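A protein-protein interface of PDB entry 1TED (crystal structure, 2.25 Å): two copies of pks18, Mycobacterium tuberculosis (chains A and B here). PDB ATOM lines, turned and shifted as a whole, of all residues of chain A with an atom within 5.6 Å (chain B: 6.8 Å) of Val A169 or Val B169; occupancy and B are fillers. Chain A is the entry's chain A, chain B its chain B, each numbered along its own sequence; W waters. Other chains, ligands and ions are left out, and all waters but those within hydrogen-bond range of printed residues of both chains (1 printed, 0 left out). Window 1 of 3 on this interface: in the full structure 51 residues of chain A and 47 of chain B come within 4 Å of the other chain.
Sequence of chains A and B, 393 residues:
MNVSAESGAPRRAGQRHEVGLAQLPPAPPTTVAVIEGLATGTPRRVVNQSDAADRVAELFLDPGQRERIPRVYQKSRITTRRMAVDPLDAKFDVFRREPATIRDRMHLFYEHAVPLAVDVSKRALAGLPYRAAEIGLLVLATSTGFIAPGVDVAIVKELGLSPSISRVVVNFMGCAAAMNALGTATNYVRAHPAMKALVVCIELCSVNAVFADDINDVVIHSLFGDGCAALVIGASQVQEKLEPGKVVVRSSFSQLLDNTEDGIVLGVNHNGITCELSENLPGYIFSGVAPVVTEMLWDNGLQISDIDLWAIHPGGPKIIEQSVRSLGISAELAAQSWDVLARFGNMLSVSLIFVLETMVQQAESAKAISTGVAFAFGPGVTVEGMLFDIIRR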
ATOM      1  N   LEU A 138     -19.871   8.493  -0.631  1.00  0.00           N
ATOM      2  CA  LEU A 138     -19.020   9.347  -1.433  1.00  0.00           C
ATOM      3  C   LEU A 138     -18.243   8.441  -2.372  1.00  0.00           C
ATOM      4  O   LEU A 138     -17.441   7.620  -1.916  1.00  0.00           O
ATOM      5  CB  LEU A 138     -18.042  10.109  -0.538  1.00  0.00           C
ATOM      6  CG  LEU A 138     -16.793  10.668  -1.222  1.00  0.00           C
ATOM      7  CD1 LEU A 138     -17.181  11.610  -2.334  1.00  0.00           C
ATOM      8  CD2 LEU A 138     -15.950  11.397  -0.204  1.00  0.00           C
ATOM      9  N   LEU A 140     -15.524   8.227  -5.365  1.00  0.00           N
ATOM     10  CA  LEU A 140     -14.483   8.998  -6.024  1.00  0.00           C
ATOM     11  C   LEU A 140     -13.851   8.171  -7.142  1.00  0.00           C
ATOM     12  O   LEU A 140     -13.367   7.064  -6.907  1.00  0.00           O
ATOM     13  CB  LEU A 140     -13.431   9.399  -4.989  1.00  0.00           C
ATOM     14  CG  LEU A 140     -12.340  10.417  -5.329  1.00  0.00           C
ATOM     15  CD1 LEU A 140     -11.330   9.800  -6.282  1.00  0.00           C
ATOM     16  CD2 LEU A 140     -12.980  11.682  -5.900  1.00  0.00           C
ATOM     17  N   ASP A 152     -10.734  11.602  -1.621  1.00  0.00           N
ATOM     18  CA  ASP A 152     -12.000  11.315  -0.935  1.00  0.00           C
ATOM     19  C   ASP A 152     -11.965  11.709   0.549  1.00  0.00           C
ATOM     20  O   ASP A 152     -12.897  12.345   1.053  1.00  0.00           O
ATOM     21  CB  ASP A 152     -12.382   9.832  -1.085  1.00  0.00           C
ATOM     22  CG  ASP A 152     -11.430   8.891  -0.362  1.00  0.00           C
ATOM     23  OD1 ASP A 152     -10.199   8.961  -0.586  1.00  0.00           O
ATOM     24  OD2 ASP A 152     -11.928   8.056   0.427  1.00  0.00           O
ATOM     25  N   ARG A 167     -17.490   5.190   1.889  1.00  0.00           N
ATOM     26  CA  ARG A 167     -16.661   5.653   0.783  1.00  0.00           C
ATOM     27  C   ARG A 167     -16.171   4.517  -0.089  1.00  0.00           C
ATOM     28  O   ARG A 167     -15.872   3.419   0.400  1.00  0.00           O
ATOM     29  CB  ARG A 167     -15.467   6.451   1.309  1.00  0.00           C
ATOM     30  CG  ARG A 167     -15.858   7.807   1.882  1.00  0.00           C
ATOM     31  CD  ARG A 167     -14.673   8.527   2.515  1.00  0.00           C
ATOM     32  NE  ARG A 167     -14.308   7.952   3.809  1.00  0.00           N
ATOM     33  CZ  ARG A 167     -13.200   7.254   4.041  1.00  0.00           C
ATOM     34  NH1 ARG A 167     -12.325   7.035   3.067  1.00  0.00           N
ATOM     35  NH2 ARG A 167     -12.976   6.769   5.254  1.00  0.00           N
ATOM     36  N   VAL A 168     -16.104   4.794  -1.388  1.00  0.00           N
ATOM     37  CA  VAL A 168     -15.648   3.837  -2.384  1.00  0.00           C
ATOM     38  C   VAL A 168     -14.785   4.562  -3.420  1.00  0.00           C
ATOM     39  O   VAL A 168     -15.224   5.523  -4.045  1.00  0.00           O
ATOM     40  CB  VAL A 168     -16.846   3.176  -3.104  1.00  0.00           C
ATOM     41  CG1 VAL A 168     -16.347   2.174  -4.145  1.00  0.00           C
ATOM     42  CG2 VAL A 168     -17.746   2.490  -2.091  1.00  0.00           C
ATOM     43  N   VAL A 169     -13.549   4.106  -3.592  1.00  0.00           N
ATOM     44  CA  VAL A 169     -12.657   4.720  -4.566  1.00  0.00           C
ATOM     45  C   VAL A 169     -12.551   3.832  -5.810  1.00  0.00           C
ATOM     46  O   VAL A 169     -12.181   2.659  -5.723  1.00  0.00           O
ATOM     47  CB  VAL A 169     -11.258   4.960  -3.962  1.00  0.00           C
ATOM     48  CG1 VAL A 169     -10.315   5.527  -5.002  1.00  0.00           C
ATOM     49  CG2 VAL A 169     -11.368   5.918  -2.810  1.00  0.00           C
ATOM     50  N   VAL A 170     -12.888   4.410  -6.960  1.00  0.00           N
ATOM     51  CA  VAL A 170     -12.867   3.708  -8.241  1.00  0.00           C
ATOM     52  C   VAL A 170     -11.740   4.189  -9.141  1.00  0.00           C
ATOM     53  O   VAL A 170     -11.818   5.273  -9.717  1.00  0.00           O
ATOM     54  CB  VAL A 170     -14.192   3.908  -8.987  1.00  0.00           C
ATOM     55  CG1 VAL A 170     -14.138   3.219 -10.343  1.00  0.00           C
ATOM     56  CG2 VAL A 170     -15.331   3.360  -8.158  1.00  0.00           C
ATOM     57  N   ASN A 171     -10.708   3.362  -9.268  1.00  0.00           N
ATOM     58  CA  ASN A 171      -9.548   3.683 -10.080  1.00  0.00           C
ATOM     59  C   ASN A 171      -9.430   2.814 -11.333  1.00  0.00           C
ATOM     60  O   ASN A 171      -9.907   1.675 -11.367  1.00  0.00           O
ATOM     61  CB  ASN A 171      -8.266   3.528  -9.256  1.00  0.00           C
ATOM     62  CG  ASN A 171      -8.193   4.500  -8.097  1.00  0.00           C
ATOM     63  OD1 ASN A 171      -8.206   5.718  -8.284  1.00  0.00           O
ATOM     64  ND2 ASN A 171      -8.114   3.963  -6.885  1.00  0.00           N
ATOM     65  N   MET A 173     -10.869   2.734 -14.289  1.00  0.00           N
ATOM     66  CA  MET A 173     -12.003   2.282 -15.070  1.00  0.00           C
ATOM     67  C   MET A 173     -12.128   3.284 -16.224  1.00  0.00           C
ATOM     68  O   MET A 173     -13.121   3.318 -16.952  1.00  0.00           O
ATOM     69  CB  MET A 173     -13.275   2.191 -14.213  1.00  0.00           C
ATOM     70  CG  MET A 173     -13.162   1.094 -13.157  1.00  0.00           C
ATOM     71  SD  MET A 173     -14.701   0.428 -12.531  1.00  0.00           S
ATOM     72  CE  MET A 173     -14.989  -0.882 -13.730  1.00  0.00           C
ATOM     73  N   LEU B 138     -19.505  -7.597 -10.210  1.00  0.00           N
ATOM     74  CA  LEU B 138     -18.205  -8.114  -9.848  1.00  0.00           C
ATOM     75  C   LEU B 138     -17.433  -6.935  -9.264  1.00  0.00           C
ATOM     76  O   LEU B 138     -17.224  -5.932  -9.947  1.00  0.00           O
ATOM     77  CB  LEU B 138     -17.458  -8.666 -11.068  1.00  0.00           C
ATOM     78  CG  LEU B 138     -15.986  -8.965 -10.773  1.00  0.00           C
ATOM     79  CD1 LEU B 138     -15.916  -9.955  -9.630  1.00  0.00           C
ATOM     80  CD2 LEU B 138     -15.283  -9.515 -11.997  1.00  0.00           C
ATOM     81  N   VAL B 139     -17.044  -7.044  -7.994  1.00  0.00           N
ATOM     82  CA  VAL B 139     -16.278  -5.991  -7.336  1.00  0.00           C
ATOM     83  C   VAL B 139     -14.878  -6.527  -7.118  1.00  0.00           C
ATOM     84  O   VAL B 139     -14.696  -7.572  -6.510  1.00  0.00           O
ATOM     85  CB  VAL B 139     -16.880  -5.599  -5.968  1.00  0.00           C
ATOM     86  CG1 VAL B 139     -16.095  -4.438  -5.376  1.00  0.00           C
ATOM     87  CG2 VAL B 139     -18.341  -5.219  -6.125  1.00  0.00           C
ATOM     88  N   LEU B 140     -13.885  -5.817  -7.628  1.00  0.00           N
ATOM     89  CA  LEU B 140     -12.502  -6.254  -7.496  1.00  0.00           C
ATOM     90  C   LEU B 140     -11.751  -5.254  -6.603  1.00  0.00           C
ATOM     91  O   LEU B 140     -11.785  -4.049  -6.854  1.00  0.00           O
ATOM     92  CB  LEU B 140     -11.878  -6.325  -8.891  1.00  0.00           C
ATOM     93  CG  LEU B 140     -10.519  -6.962  -9.212  1.00  0.00           C
ATOM     94  CD1 LEU B 140      -9.408  -6.134  -8.595  1.00  0.00           C
ATOM     95  CD2 LEU B 140     -10.483  -8.404  -8.733  1.00  0.00           C
ATOM     96  N   ALA B 141     -11.104  -5.753  -5.550  1.00  0.00           N
ATOM     97  CA  ALA B 141     -10.346  -4.892  -4.638  1.00  0.00           C
ATOM     98  C   ALA B 141      -8.867  -5.282  -4.579  1.00  0.00           C
ATOM     99  O   ALA B 141      -8.520  -6.456  -4.424  1.00  0.00           O
ATOM    100  CB  ALA B 141     -10.956  -4.935  -3.227  1.00  0.00           C
ATOM    101  N   THR B 142      -8.000  -4.283  -4.706  1.00  0.00           N
ATOM    102  CA  THR B 142      -6.563  -4.495  -4.654  1.00  0.00           C
ATOM    103  C   THR B 142      -5.870  -3.179  -4.354  1.00  0.00           C
ATOM    104  O   THR B 142      -6.402  -2.111  -4.661  1.00  0.00           O
ATOM    105  CB  THR B 142      -5.995  -4.978  -5.998  1.00  0.00           C
ATOM    106  OG1 THR B 142      -6.813  -6.030  -6.511  1.00  0.00           O
ATOM    107  CG2 THR B 142      -4.565  -5.484  -5.817  1.00  0.00           C
ATOM    108  N   GLY B 145      -1.600  -3.727  -7.254  1.00  0.00           N
ATOM    109  CA  GLY B 145      -1.413  -3.823  -8.694  1.00  0.00           C
ATOM    110  C   GLY B 145      -2.381  -2.961  -9.486  1.00  0.00           C
ATOM    111  O   GLY B 145      -3.587  -2.969  -9.216  1.00  0.00           O
ATOM    112  N   ILE B 147      -3.518  -2.086 -13.449  1.00  0.00           N
ATOM    113  CA  ILE B 147      -3.524  -2.351 -14.897  1.00  0.00           C
ATOM    114  C   ILE B 147      -4.945  -2.449 -15.425  1.00  0.00           C
ATOM    115  O   ILE B 147      -5.835  -2.964 -14.749  1.00  0.00           O
ATOM    116  CB  ILE B 147      -2.838  -3.692 -15.296  1.00  0.00           C
ATOM    117  CG1 ILE B 147      -2.826  -4.643 -14.113  1.00  0.00           C
ATOM    118  CG2 ILE B 147      -1.489  -3.435 -15.922  1.00  0.00           C
ATOM    119  CD1 ILE B 147      -4.174  -5.299 -13.872  1.00  0.00           C
ATOM    120  N   GLY B 150      -8.006  -5.164 -16.235  1.00  0.00           N
ATOM    121  CA  GLY B 150      -7.419  -5.952 -15.170  1.00  0.00           C
ATOM    122  C   GLY B 150      -8.010  -7.312 -14.861  1.00  0.00           C
ATOM    123  O   GLY B 150      -8.700  -7.920 -15.677  1.00  0.00           O
ATOM    124  N   ASP B 152     -10.467  -8.202 -13.153  1.00  0.00           N
ATOM    125  CA  ASP B 152     -11.922  -8.302 -13.240  1.00  0.00           C
ATOM    126  C   ASP B 152     -12.364  -8.697 -14.652  1.00  0.00           C
ATOM    127  O   ASP B 152     -13.282  -9.495 -14.824  1.00  0.00           O
ATOM    128  CB  ASP B 152     -12.576  -6.974 -12.848  1.00  0.00           C
ATOM    129  CG  ASP B 152     -12.203  -5.844 -13.785  1.00  0.00           C
ATOM    130  OD1 ASP B 152     -10.993  -5.576 -13.936  1.00  0.00           O
ATOM    131  OD2 ASP B 152     -13.119  -5.226 -14.369  1.00  0.00           O
ATOM    132  N   ARG B 167     -19.372  -3.932 -13.123  1.00  0.00           N
ATOM    133  CA  ARG B 167     -18.055  -4.055 -12.519  1.00  0.00           C
ATOM    134  C   ARG B 167     -17.525  -2.766 -11.895  1.00  0.00           C
ATOM    135  O   ARG B 167     -17.717  -1.676 -12.430  1.00  0.00           O
ATOM    136  CB  ARG B 167     -17.059  -4.562 -13.562  1.00  0.00           C
ATOM    137  CG  ARG B 167     -17.275  -6.019 -13.920  1.00  0.00           C
ATOM    138  CD  ARG B 167     -16.352  -6.491 -15.013  1.00  0.00           C
ATOM    139  NE  ARG B 167     -16.630  -5.812 -16.272  1.00  0.00           N
ATOM    140  CZ  ARG B 167     -15.908  -4.812 -16.763  1.00  0.00           C
ATOM    141  NH1 ARG B 167     -14.844  -4.360 -16.107  1.00  0.00           N
ATOM    142  NH2 ARG B 167     -16.259  -4.258 -17.912  1.00  0.00           N
ATOM    143  N   VAL B 168     -16.872  -2.903 -10.744  1.00  0.00           N
ATOM    144  CA  VAL B 168     -16.274  -1.765 -10.060  1.00  0.00           C
ATOM    145  C   VAL B 168     -14.958  -2.238  -9.481  1.00  0.00           C
ATOM    146  O   VAL B 168     -14.897  -3.282  -8.829  1.00  0.00           O
ATOM    147  CB  VAL B 168     -17.132  -1.237  -8.891  1.00  0.00           C
ATOM    148  CG1 VAL B 168     -16.595   0.114  -8.446  1.00  0.00           C
ATOM    149  CG2 VAL B 168     -18.578  -1.131  -9.301  1.00  0.00           C
ATOM    150  N   VAL B 169     -13.905  -1.474  -9.740  1.00  0.00           N
ATOM    151  CA  VAL B 169     -12.583  -1.805  -9.238  1.00  0.00           C
ATOM    152  C   VAL B 169     -12.217  -0.849  -8.107  1.00  0.00           C
ATOM    153  O   VAL B 169     -12.101   0.363  -8.305  1.00  0.00           O
ATOM    154  CB  VAL B 169     -11.528  -1.700 -10.350  1.00  0.00           C
ATOM    155  CG1 VAL B 169     -10.148  -2.084  -9.802  1.00  0.00           C
ATOM    156  CG2 VAL B 169     -11.918  -2.602 -11.510  1.00  0.00           C
ATOM    157  N   VAL B 170     -12.041  -1.409  -6.917  1.00  0.00           N
ATOM    158  CA  VAL B 170     -11.699  -0.633  -5.725  1.00  0.00           C
ATOM    159  C   VAL B 170     -10.204  -0.742  -5.442  1.00  0.00           C
ATOM    160  O   VAL B 170      -9.729  -1.786  -4.998  1.00  0.00           O
ATOM    161  CB  VAL B 170     -12.484  -1.164  -4.516  1.00  0.00           C
ATOM    162  CG1 VAL B 170     -12.262  -0.267  -3.306  1.00  0.00           C
ATOM    163  CG2 VAL B 170     -13.961  -1.254  -4.870  1.00  0.00           C
ATOM    164  N   ASN B 171      -9.470   0.335  -5.710  1.00  0.00           N
ATOM    165  CA  ASN B 171      -8.026   0.352  -5.506  1.00  0.00           C
ATOM    166  C   ASN B 171      -7.574   1.304  -4.405  1.00  0.00           C
ATOM    167  O   ASN B 171      -8.204   2.325  -4.154  1.00  0.00           O
ATOM    168  CB  ASN B 171      -7.294   0.749  -6.798  1.00  0.00           C
ATOM    169  CG  ASN B 171      -7.385  -0.311  -7.888  1.00  0.00           C
ATOM    170  OD1 ASN B 171      -7.106  -1.494  -7.658  1.00  0.00           O
ATOM    171  ND2 ASN B 171      -7.756   0.115  -9.093  1.00  0.00           N
ATOM    172  N   PHE B 172      -6.465   0.947  -3.766  1.00  0.00           N
ATOM    173  CA  PHE B 172      -5.856   1.739  -2.710  1.00  0.00           C
ATOM    174  C   PHE B 172      -6.682   2.027  -1.464  1.00  0.00           C
ATOM    175  O   PHE B 172      -6.490   3.063  -0.814  1.00  0.00           O
ATOM    176  CB  PHE B 172      -5.318   3.051  -3.297  1.00  0.00           C
ATOM    177  CG  PHE B 172      -3.812   3.085  -3.412  1.00  0.00           C
ATOM    178  CD1 PHE B 172      -3.080   1.903  -3.466  1.00  0.00           C
ATOM    179  CD2 PHE B 172      -3.132   4.296  -3.503  1.00  0.00           C
ATOM    180  CE1 PHE B 172      -1.706   1.924  -3.609  1.00  0.00           C
ATOM    181  CE2 PHE B 172      -1.748   4.328  -3.649  1.00  0.00           C
ATOM    182  CZ  PHE B 172      -1.034   3.142  -3.703  1.00  0.00           C
ATOM    183  N   MET B 173      -7.592   1.116  -1.130  1.00  0.00           N
ATOM    184  CA  MET B 173      -8.397   1.265   0.073  1.00  0.00           C
ATOM    185  C   MET B 173      -7.786   0.368   1.158  1.00  0.00           C
ATOM    186  O   MET B 173      -8.351   0.158   2.229  1.00  0.00           O
ATOM    187  CB  MET B 173      -9.871   0.936  -0.212  1.00  0.00           C
ATOM    188  CG  MET B 173     -10.500   1.979  -1.147  1.00  0.00           C
ATOM    189  SD  MET B 173     -12.247   2.334  -0.908  1.00  0.00           S
ATOM    190  CE  MET B 173     -12.199   3.477   0.522  1.00  0.00           C
ATOM    191  N   ASN B 180     -15.293  -2.274   2.086  1.00  0.00           N
ATOM    192  CA  ASN B 180     -15.788  -1.278   1.148  1.00  0.00           C
ATOM    193  C   ASN B 180     -16.396  -2.023  -0.045  1.00  0.00           C
ATOM    194  O   ASN B 180     -17.434  -1.627  -0.590  1.00  0.00           O
ATOM    195  CB  ASN B 180     -14.642  -0.388   0.665  1.00  0.00           C
ATOM    196  CG  ASN B 180     -14.074   0.480   1.768  1.00  0.00           C
ATOM    197  OD1 ASN B 180     -14.664   1.503   2.141  1.00  0.00           O
ATOM    198  ND2 ASN B 180     -12.934   0.071   2.307  1.00  0.00           N
HETATM  199  O   HOH W   1     -16.417   3.824   3.900  1.00  0.00           O
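Water W1 lies within hydrogen-bond range of the backbone NH of Arg A167 (2.7 Å) and the side-chain amide oxygen of Asn B180 (3.4 Å).
Among the printed residues, merely in contact across the chains: Val A169 with Val B170 (3.3 Å), Val A170 with Val B169 (3.4 Å), Val A170 with Val B168 (3.5 Å), Val A169 with Asn B171 (3.6 Å), Met A173 with Val B168 (3.7 Å) and Arg A167 with Met B173 (3.7 Å).
Arg A167 touches Met B173, and with the chains exchanged Met A173 touches Arg B167.
Val A169 touches Val B170, and with the chains exchanged Val A170 touches Val B169.
Val A169 touches Asn B171, and with the chains exchanged Asn A171 touches Val B169.
Asn B171 touches its own counterpart, Asn A171.
Positions printed for both chains: 138, 140, 152, 167, 168, 169, 170, 171 and 173.
The backbone NH of Val A169 sits at hydrogen-bond distance from the side-chain sulfur of Met B173 (3.5 Å).
O of Arg B167 sits close to SD of Met A173, 3.7 Å away.
The backbone carbonyl oxygen (O) of Val B169 lies close to the backbone carbonyl oxygen (O) of Val A169 (3.5 Å).
O of Asn B171 is in hydrogen-bond range of ND2 of Asn A171 (3.2 Å).
The side-chain sulfur (SD) of Met A173 sits at hydrogen-bond distance from the backbone NH (N) of Val B169, at 3.5 Å.
The side-chain amide oxygen (OD1) of Asn B180 lies close to the backbone carbonyl oxygen (O) of Arg A167.
The backbone carbonyl oxygen of Val B169 sits at hydrogen-bond distance from the backbone NH of Asn A171, at 3.4 Å.
The backbone NH (N) of Leu B140 is in hydrogen-bond range of the backbone carbonyl oxygen (O) of Val B168.
The backbone carbonyl oxygen (O) of Leu B138 is in hydrogen-bond range of the backbone NH (N) of Val B168.
The backbone carbonyl oxygen (O) of Thr B142 lies close to the side-chain amide oxygen (OD1) of Asn B171 (3.1 Å).
The backbone NH of Val B170 sits at hydrogen-bond distance from the backbone carbonyl oxygen of Leu B140 (2.7 Å).
O of Val B170 is in hydrogen-bond range of N of Thr B142, 3.1 Å away.
The backbone NH of Val A170 lies within hydrogen-bond range of the backbone carbonyl oxygen of Leu A140 (2.7 Å).
Printed residues of chain B that touch a printed residue of chain A: Arg B167, Val B168, Val B169, Val B170, Asn B171, Met B173 and Asn B180.
Hydrophobic or aromatic side chains of chain B that line the printed part of chain A: Val B168, Val B169, Val B170 and Met B173.
Hydrophobic or aromatic side chains of chain A within 4 Å of the printed part of chain B: Val A169, Val A170 and Met A173.
Printed residues of chain B within 4 Å of Val A169: Val B169 (3.5 Å), Val B170 (3.3 Å), Asn B171 (3.6 Å) and Met B173 (3.5 Å).
Val B169 touches four residues of chain A.
Of the printed residues of chain A, Asn B180 touches Arg A167 (2.9 Å).
Printed residues of chain B within 4 Å of Arg A167: Met B173 (3.7 Å) and Asn B180 (2.9 Å).
Of the printed residues of chain A, Val B168 touches Val A170 (3.5 Å) and Met A173 (3.7 Å).
The nearest residue of chain B that does not touch Val A169 is Val B168 (5.8 Å).
The nearest printed residue of chain A that does not touch Val B169 is Val A168 (6.2 Å).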
